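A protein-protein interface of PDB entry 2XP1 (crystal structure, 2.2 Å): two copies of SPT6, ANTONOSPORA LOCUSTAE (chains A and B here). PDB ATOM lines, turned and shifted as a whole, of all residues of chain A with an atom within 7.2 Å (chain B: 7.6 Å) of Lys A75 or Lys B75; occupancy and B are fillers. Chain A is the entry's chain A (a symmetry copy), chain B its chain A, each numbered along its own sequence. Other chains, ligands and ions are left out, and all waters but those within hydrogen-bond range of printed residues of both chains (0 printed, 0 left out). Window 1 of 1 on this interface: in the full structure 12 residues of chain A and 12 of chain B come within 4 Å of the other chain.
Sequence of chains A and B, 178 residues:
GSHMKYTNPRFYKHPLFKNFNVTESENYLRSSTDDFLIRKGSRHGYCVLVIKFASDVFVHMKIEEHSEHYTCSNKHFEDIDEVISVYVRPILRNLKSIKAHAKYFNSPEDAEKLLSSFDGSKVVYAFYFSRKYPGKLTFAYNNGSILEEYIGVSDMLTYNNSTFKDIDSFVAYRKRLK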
ATOM      1  N   TYR A  70      24.958  15.925   8.799  1.00  0.00           N
ATOM      2  CA  TYR A  70      23.646  15.546   8.333  1.00  0.00           C
ATOM      3  C   TYR A  70      23.577  14.007   8.362  1.00  0.00           C
ATOM      4  O   TYR A  70      24.611  13.343   8.406  1.00  0.00           O
ATOM      5  CB  TYR A  70      23.416  16.108   6.905  1.00  0.00           C
ATOM      6  CG  TYR A  70      23.388  17.642   6.849  1.00  0.00           C
ATOM      7  CD1 TYR A  70      24.572  18.392   6.866  1.00  0.00           C
ATOM      8  CD2 TYR A  70      22.187  18.329   6.830  1.00  0.00           C
ATOM      9  CE1 TYR A  70      24.545  19.786   6.850  1.00  0.00           C
ATOM     10  CE2 TYR A  70      22.151  19.719   6.819  1.00  0.00           C
ATOM     11  CZ  TYR A  70      23.328  20.432   6.815  1.00  0.00           C
ATOM     12  OH  TYR A  70      23.279  21.805   6.818  1.00  0.00           O
ATOM     13  N   THR A  71      22.360  13.455   8.353  1.00  0.00           N
ATOM     14  CA  THR A  71      22.165  12.038   8.088  1.00  0.00           C
ATOM     15  C   THR A  71      21.154  11.861   6.994  1.00  0.00           C
ATOM     16  O   THR A  71      20.192  12.625   6.894  1.00  0.00           O
ATOM     17  CB  THR A  71      21.668  11.250   9.300  1.00  0.00           C
ATOM     18  OG1 THR A  71      20.446  11.836   9.759  1.00  0.00           O
ATOM     19  CG2 THR A  71      22.690  11.271  10.369  1.00  0.00           C
ATOM     20  N   CYS A  72      21.392  10.851   6.167  1.00  0.00           N
ATOM     21  CA  CYS A  72      20.480  10.487   5.078  1.00  0.00           C
ATOM     22  C   CYS A  72      20.605   8.987   4.865  1.00  0.00           C
ATOM     23  O   CYS A  72      21.723   8.455   4.796  1.00  0.00           O
ATOM     24  CB  CYS A  72      20.848  11.195   3.777  1.00  0.00           C
ATOM     25  SG  CYS A  72      19.561  10.983   2.494  1.00  0.00           S
ATOM     26  N   SER A  73      19.466   8.303   4.764  1.00  0.00           N
ATOM     27  CA  SER A  73      19.421   6.814   4.703  1.00  0.00           C
ATOM     28  C   SER A  73      20.402   6.070   5.619  1.00  0.00           C
ATOM     29  O   SER A  73      21.177   5.204   5.180  1.00  0.00           O
ATOM     30  CB  SER A  73      19.509   6.370   3.269  1.00  0.00           C
ATOM     31  OG  SER A  73      18.447   7.039   2.560  1.00  0.00           O
ATOM     32  N   ASN A  74      20.356   6.434   6.902  1.00  0.00           N
ATOM     33  CA  ASN A  74      21.140   5.777   7.965  1.00  0.00           C
ATOM     34  C   ASN A  74      22.654   6.011   7.898  1.00  0.00           C
ATOM     35  O   ASN A  74      23.399   5.478   8.702  1.00  0.00           O
ATOM     36  CB  ASN A  74      20.808   4.272   8.026  1.00  0.00           C
ATOM     37  CG  ASN A  74      19.329   4.019   8.326  1.00  0.00           C
ATOM     38  OD1 ASN A  74      18.807   4.463   9.372  1.00  0.00           O
ATOM     39  ND2 ASN A  74      18.642   3.316   7.408  1.00  0.00           N
ATOM     40  N   LYS A  75      23.077   6.796   6.915  1.00  0.00           N
ATOM     41  CA  LYS A  75      24.457   7.118   6.662  1.00  0.00           C
ATOM     42  C   LYS A  75      24.669   8.530   7.226  1.00  0.00           C
ATOM     43  O   LYS A  75      23.732   9.319   7.374  1.00  0.00           O
ATOM     44  CB  LYS A  75      24.752   7.100   5.137  1.00  0.00           C
ATOM     45  CG  LYS A  75      24.991   5.708   4.465  1.00  0.00           C
ATOM     46  CD  LYS A  75      26.454   5.171   4.674  1.00  0.00           C
ATOM     47  CE  LYS A  75      26.744   3.722   4.121  1.00  0.00           C
ATOM     48  NZ  LYS A  75      28.171   3.244   4.384  1.00  0.00           N
ATOM     49  N   HIS A  76      25.917   8.858   7.484  1.00  0.00           N
ATOM     50  CA  HIS A  76      26.256  10.108   8.097  1.00  0.00           C
ATOM     51  C   HIS A  76      27.056  10.959   7.105  1.00  0.00           C
ATOM     52  O   HIS A  76      27.904  10.404   6.432  1.00  0.00           O
ATOM     53  CB  HIS A  76      27.100   9.715   9.305  1.00  0.00           C
ATOM     54  CG  HIS A  76      27.733  10.860  10.002  1.00  0.00           C
ATOM     55  ND1 HIS A  76      29.029  11.253   9.747  1.00  0.00           N
ATOM     56  CD2 HIS A  76      27.268  11.676  10.977  1.00  0.00           C
ATOM     57  CE1 HIS A  76      29.334  12.265  10.536  1.00  0.00           C
ATOM     58  NE2 HIS A  76      28.290  12.531  11.302  1.00  0.00           N
ATOM     59  N   PHE A  77      26.814  12.275   7.019  1.00  0.00           N
ATOM     60  CA  PHE A  77      27.523  13.157   6.059  1.00  0.00           C
ATOM     61  C   PHE A  77      28.025  14.457   6.653  1.00  0.00           C
ATOM     62  O   PHE A  77      27.298  15.119   7.376  1.00  0.00           O
ATOM     63  CB  PHE A  77      26.595  13.489   4.893  1.00  0.00           C
ATOM     64  CG  PHE A  77      26.019  12.294   4.267  1.00  0.00           C
ATOM     65  CD1 PHE A  77      24.825  11.764   4.737  1.00  0.00           C
ATOM     66  CD2 PHE A  77      26.710  11.633   3.250  1.00  0.00           C
ATOM     67  CE1 PHE A  77      24.284  10.595   4.174  1.00  0.00           C
ATOM     68  CE2 PHE A  77      26.183  10.438   2.657  1.00  0.00           C
ATOM     69  CZ  PHE A  77      24.959   9.936   3.113  1.00  0.00           C
ATOM     70  N   VAL A  83      26.421  14.703   0.918  1.00  0.00           N
ATOM     71  CA  VAL A  83      25.214  13.890   0.557  1.00  0.00           C
ATOM     72  C   VAL A  83      25.154  13.740  -0.963  1.00  0.00           C
ATOM     73  O   VAL A  83      24.980  12.634  -1.500  1.00  0.00           O
ATOM     74  CB  VAL A  83      23.880  14.523   1.072  1.00  0.00           C
ATOM     75  CG1 VAL A  83      22.669  13.804   0.542  1.00  0.00           C
ATOM     76  CG2 VAL A  83      23.841  14.543   2.553  1.00  0.00           C
ATOM     77  N   VAL A  86      28.572  11.736  -2.369  1.00  0.00           N
ATOM     78  CA  VAL A  86      28.688  10.394  -1.836  1.00  0.00           C
ATOM     79  C   VAL A  86      27.439   9.607  -2.103  1.00  0.00           C
ATOM     80  O   VAL A  86      27.511   8.414  -2.295  1.00  0.00           O
ATOM     81  CB  VAL A  86      29.074  10.380  -0.321  1.00  0.00           C
ATOM     82  CG1 VAL A  86      28.843   9.017   0.295  1.00  0.00           C
ATOM     83  CG2 VAL A  86      30.513  10.758  -0.151  1.00  0.00           C
ATOM     84  N   TYR A  87      26.295  10.278  -2.168  1.00  0.00           N
ATOM     85  CA  TYR A  87      25.024   9.569  -2.167  1.00  0.00           C
ATOM     86  C   TYR A  87      24.198   9.745  -3.426  1.00  0.00           C
ATOM     87  O   TYR A  87      23.825   8.751  -4.060  1.00  0.00           O
ATOM     88  CB  TYR A  87      24.247   9.904  -0.890  1.00  0.00           C
ATOM     89  CG  TYR A  87      23.009   9.100  -0.710  1.00  0.00           C
ATOM     90  CD1 TYR A  87      23.079   7.746  -0.361  1.00  0.00           C
ATOM     91  CD2 TYR A  87      21.767   9.678  -0.885  1.00  0.00           C
ATOM     92  CE1 TYR A  87      21.928   6.988  -0.186  1.00  0.00           C
ATOM     93  CE2 TYR A  87      20.602   8.936  -0.722  1.00  0.00           C
ATOM     94  CZ  TYR A  87      20.691   7.582  -0.362  1.00  0.00           C
ATOM     95  OH  TYR A  87      19.524   6.826  -0.205  1.00  0.00           O
ATOM     96  N   GLU B  64      32.658   7.268  16.791  1.00  0.00           N
ATOM     97  CA  GLU B  64      32.668   8.670  17.174  1.00  0.00           C
ATOM     98  C   GLU B  64      31.452   9.068  17.993  1.00  0.00           C
ATOM     99  O   GLU B  64      30.329   8.633  17.719  1.00  0.00           O
ATOM    100  CB  GLU B  64      32.821   9.575  15.952  1.00  0.00           C
ATOM    101  CG  GLU B  64      34.168   9.399  15.275  1.00  0.00           C
ATOM    102  CD  GLU B  64      34.619  10.664  14.580  1.00  0.00           C
ATOM    103  OE1 GLU B  64      34.730  11.683  15.295  1.00  0.00           O
ATOM    104  OE2 GLU B  64      34.854  10.646  13.330  1.00  0.00           O
ATOM    105  N   HIS B  66      29.160  12.139  19.116  1.00  0.00           N
ATOM    106  CA  HIS B  66      28.717  13.479  18.800  1.00  0.00           C
ATOM    107  C   HIS B  66      27.664  13.803  19.824  1.00  0.00           C
ATOM    108  O   HIS B  66      27.423  12.994  20.715  1.00  0.00           O
ATOM    109  CB  HIS B  66      28.168  13.550  17.363  1.00  0.00           C
ATOM    110  CG  HIS B  66      29.167  13.137  16.327  1.00  0.00           C
ATOM    111  ND1 HIS B  66      28.866  12.266  15.304  1.00  0.00           N
ATOM    112  CD2 HIS B  66      30.481  13.439  16.189  1.00  0.00           C
ATOM    113  CE1 HIS B  66      29.944  12.071  14.563  1.00  0.00           C
ATOM    114  NE2 HIS B  66      30.939  12.766  15.082  1.00  0.00           N
ATOM    115  N   TYR B  70      26.061   8.600  17.723  1.00  0.00           N
ATOM    116  CA  TYR B  70      27.386   8.092  17.460  1.00  0.00           C
ATOM    117  C   TYR B  70      27.481   7.825  15.946  1.00  0.00           C
ATOM    118  O   TYR B  70      26.457   7.723  15.271  1.00  0.00           O
ATOM    119  CB  TYR B  70      27.626   6.804  18.290  1.00  0.00           C
ATOM    120  CG  TYR B  70      27.629   7.045  19.806  1.00  0.00           C
ATOM    121  CD1 TYR B  70      26.433   7.186  20.522  1.00  0.00           C
ATOM    122  CD2 TYR B  70      28.819   7.179  20.501  1.00  0.00           C
ATOM    123  CE1 TYR B  70      26.437   7.440  21.894  1.00  0.00           C
ATOM    124  CE2 TYR B  70      28.831   7.436  21.867  1.00  0.00           C
ATOM    125  CZ  TYR B  70      27.643   7.550  22.551  1.00  0.00           C
ATOM    126  OH  TYR B  70      27.668   7.819  23.898  1.00  0.00           O
ATOM    127  N   THR B  71      28.707   7.731  15.422  1.00  0.00           N
ATOM    128  CA  THR B  71      28.929   7.200  14.086  1.00  0.00           C
ATOM    129  C   THR B  71      29.959   6.110  14.137  1.00  0.00           C
ATOM    130  O   THR B  71      30.909   6.175  14.920  1.00  0.00           O
ATOM    131  CB  THR B  71      29.423   8.246  13.085  1.00  0.00           C
ATOM    132  OG1 THR B  71      30.629   8.830  13.590  1.00  0.00           O
ATOM    133  CG2 THR B  71      28.386   9.281  12.885  1.00  0.00           C
ATOM    134  N   CYS B  72      29.749   5.100  13.303  1.00  0.00           N
ATOM    135  CA  CYS B  72      30.682   3.976  13.169  1.00  0.00           C
ATOM    136  C   CYS B  72      30.585   3.476  11.737  1.00  0.00           C
ATOM    137  O   CYS B  72      29.478   3.287  11.212  1.00  0.00           O
ATOM    138  CB  CYS B  72      30.321   2.831  14.110  1.00  0.00           C
ATOM    139  SG  CYS B  72      31.628   1.553  14.167  1.00  0.00           S
ATOM    140  N   SER B  73      31.737   3.265  11.101  1.00  0.00           N
ATOM    141  CA  SER B  73      31.808   2.919   9.652  1.00  0.00           C
ATOM    142  C   SER B  73      30.827   3.657   8.732  1.00  0.00           C
ATOM    143  O   SER B  73      30.073   3.046   7.956  1.00  0.00           O
ATOM    144  CB  SER B  73      31.748   1.424   9.493  1.00  0.00           C
ATOM    145  OG  SER B  73      32.808   0.875  10.301  1.00  0.00           O
ATOM    146  N   ASN B  74      30.849   4.987   8.842  1.00  0.00           N
ATOM    147  CA  ASN B  74      30.062   5.889   7.981  1.00  0.00           C
ATOM    148  C   ASN B  74      28.545   5.843   8.203  1.00  0.00           C
ATOM    149  O   ASN B  74      27.798   6.517   7.514  1.00  0.00           O
ATOM    150  CB  ASN B  74      30.418   5.665   6.497  1.00  0.00           C
ATOM    151  CG  ASN B  74      31.897   5.936   6.212  1.00  0.00           C
ATOM    152  OD1 ASN B  74      32.397   7.056   6.453  1.00  0.00           O
ATOM    153  ND2 ASN B  74      32.608   4.911   5.709  1.00  0.00           N
ATOM    154  N   LYS B  75      28.123   5.023   9.157  1.00  0.00           N
ATOM    155  CA  LYS B  75      26.741   4.814   9.503  1.00  0.00           C
ATOM    156  C   LYS B  75      26.497   5.636  10.776  1.00  0.00           C
ATOM    157  O   LYS B  75      27.419   5.949  11.534  1.00  0.00           O
ATOM    158  CB  LYS B  75      26.467   3.309   9.775  1.00  0.00           C
ATOM    159  CG  LYS B  75      26.261   2.377   8.536  1.00  0.00           C
ATOM    160  CD  LYS B  75      24.805   2.455   7.948  1.00  0.00           C
ATOM    161  CE  LYS B  75      24.547   1.628   6.630  1.00  0.00           C
ATOM    162  NZ  LYS B  75      23.125   1.769   6.090  1.00  0.00           N
ATOM    163  N   HIS B  76      25.240   5.931  11.031  1.00  0.00           N
ATOM    164  CA  HIS B  76      24.872   6.768  12.134  1.00  0.00           C
ATOM    165  C   HIS B  76      24.072   5.946  13.150  1.00  0.00           C
ATOM    166  O   HIS B  76      23.243   5.163  12.723  1.00  0.00           O
ATOM    167  CB  HIS B  76      24.018   7.863  11.504  1.00  0.00           C
ATOM    168  CG  HIS B  76      23.357   8.757  12.484  1.00  0.00           C
ATOM    169  ND1 HIS B  76      22.058   8.561  12.900  1.00  0.00           N
ATOM    170  CD2 HIS B  76      23.794   9.879  13.102  1.00  0.00           C
ATOM    171  CE1 HIS B  76      21.724   9.525  13.737  1.00  0.00           C
ATOM    172  NE2 HIS B  76      22.753  10.345  13.864  1.00  0.00           N
ATOM    173  N   PHE B  77      24.292   6.119  14.461  1.00  0.00           N
ATOM    174  CA  PHE B  77      23.583   5.336  15.502  1.00  0.00           C
ATOM    175  C   PHE B  77      23.050   6.160  16.655  1.00  0.00           C
ATOM    176  O   PHE B  77      23.755   7.010  17.175  1.00  0.00           O
ATOM    177  CB  PHE B  77      24.520   4.271  16.065  1.00  0.00           C
ATOM    178  CG  PHE B  77      25.125   3.436  15.022  1.00  0.00           C
ATOM    179  CD1 PHE B  77      26.321   3.816  14.428  1.00  0.00           C
ATOM    180  CD2 PHE B  77      24.459   2.299  14.560  1.00  0.00           C
ATOM    181  CE1 PHE B  77      26.890   3.046  13.397  1.00  0.00           C
ATOM    182  CE2 PHE B  77      25.015   1.496  13.510  1.00  0.00           C
ATOM    183  CZ  PHE B  77      26.240   1.867  12.946  1.00  0.00           C
ATOM    184  N   VAL B  83      24.729   0.608  18.026  1.00  0.00           N
ATOM    185  CA  VAL B  83      25.955   0.118  17.315  1.00  0.00           C
ATOM    186  C   VAL B  83      26.038  -1.402  17.462  1.00  0.00           C
ATOM    187  O   VAL B  83      26.238  -2.139  16.483  1.00  0.00           O
ATOM    188  CB  VAL B  83      27.270   0.767  17.854  1.00  0.00           C
ATOM    189  CG1 VAL B  83      28.500   0.130  17.268  1.00  0.00           C
ATOM    190  CG2 VAL B  83      27.289   2.225  17.589  1.00  0.00           C
ATOM    191  N   VAL B  86      22.674  -3.225  15.720  1.00  0.00           N
ATOM    192  CA  VAL B  86      22.574  -2.963  14.298  1.00  0.00           C
ATOM    193  C   VAL B  86      23.840  -3.356  13.595  1.00  0.00           C
ATOM    194  O   VAL B  86      23.790  -3.776  12.461  1.00  0.00           O
ATOM    195  CB  VAL B  86      22.167  -1.486  13.987  1.00  0.00           C
ATOM    196  CG1 VAL B  86      22.413  -1.140  12.535  1.00  0.00           C
ATOM    197  CG2 VAL B  86      20.719  -1.271  14.305  1.00  0.00           C
ATOM    198  N   TYR B  87      24.973  -3.270  14.282  1.00  0.00           N
ATOM    199  CA  TYR B  87      26.255  -3.385  13.604  1.00  0.00           C
ATOM    200  C   TYR B  87      27.095  -4.572  14.031  1.00  0.00           C
ATOM    201  O   TYR B  87      27.494  -5.380  13.184  1.00  0.00           O
ATOM    202  CB  TYR B  87      27.008  -2.054  13.697  1.00  0.00           C
ATOM    203  CG  TYR B  87      28.258  -2.012  12.890  1.00  0.00           C
ATOM    204  CD1 TYR B  87      28.205  -1.932  11.494  1.00  0.00           C
ATOM    205  CD2 TYR B  87      29.492  -2.051  13.509  1.00  0.00           C
ATOM    206  CE1 TYR B  87      29.366  -1.887  10.733  1.00  0.00           C
ATOM    207  CE2 TYR B  87      30.667  -2.015  12.765  1.00  0.00           C
ATOM    208  CZ  TYR B  87      30.596  -1.924  11.366  1.00  0.00           C
ATOM    209  OH  TYR B  87      31.772  -1.896  10.611  1.00  0.00           O
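Tyr A70 touches none of the printed residues of chain B.
Lys A75 touches two residues of chain B.
Of the printed residues of chain A, His B66 touches His A76.
Printed residues of chain A within 4 Å of Asn B74: Lys A75 (3.4 Å) and His A76 (3.0 Å).
Of chain A, only Asn A74 (3.4 Å) and Lys A75 (3.9 Å) come within 4 Å of Lys B75.
The nearest residue of chain B that does not touch Lys A75 is Ser B73 (4.1 Å).
The nearest residue of chain A that does not touch Lys B75 is Ser A73 (4.1 Å).
O of Thr B71 sits at hydrogen-bond distance from N of Glu B64 (2.8 Å).
The backbone carbonyl oxygen (O) of Asn B74 is in hydrogen-bond range of the backbone NH (N) of His A76 (3.0 Å).
The backbone NH (N) of His B76 sits at hydrogen-bond distance from the backbone carbonyl oxygen (O) of Asn A74 (3.0 Å).
Among the printed residues, pairs that only touch across the chains: Thr A71 with His B76 (3.3 Å), His A76 with Thr B71 (3.3 Å), Lys A75 with Asn B74 (3.4 Å), Asn A74 with Lys B75 (3.4 Å), His A76 with His B66 (3.7 Å) and Lys A75 with Lys B75 (3.9 Å).
Hydrophobic or aromatic side chains of chain B within 4 Å of the printed part of chain A: His B66 and His B76.
Of the 11 printed residues of chain A, 4 touch a printed residue of chain B.
Hydrophobic or aromatic side chains of chain A that line the printed part of chain B: His A76.
Thr A71 touches His B76, and with the chains exchanged His A76 touches Thr B71.
Asn A74 touches Lys B75, and with the chains exchanged Lys A75 touches Asn B74.
Asn A74 touches His B76, and with the chains exchanged His A76 touches Asn B74.
Lys B75 touches its own counterpart, Lys A75.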
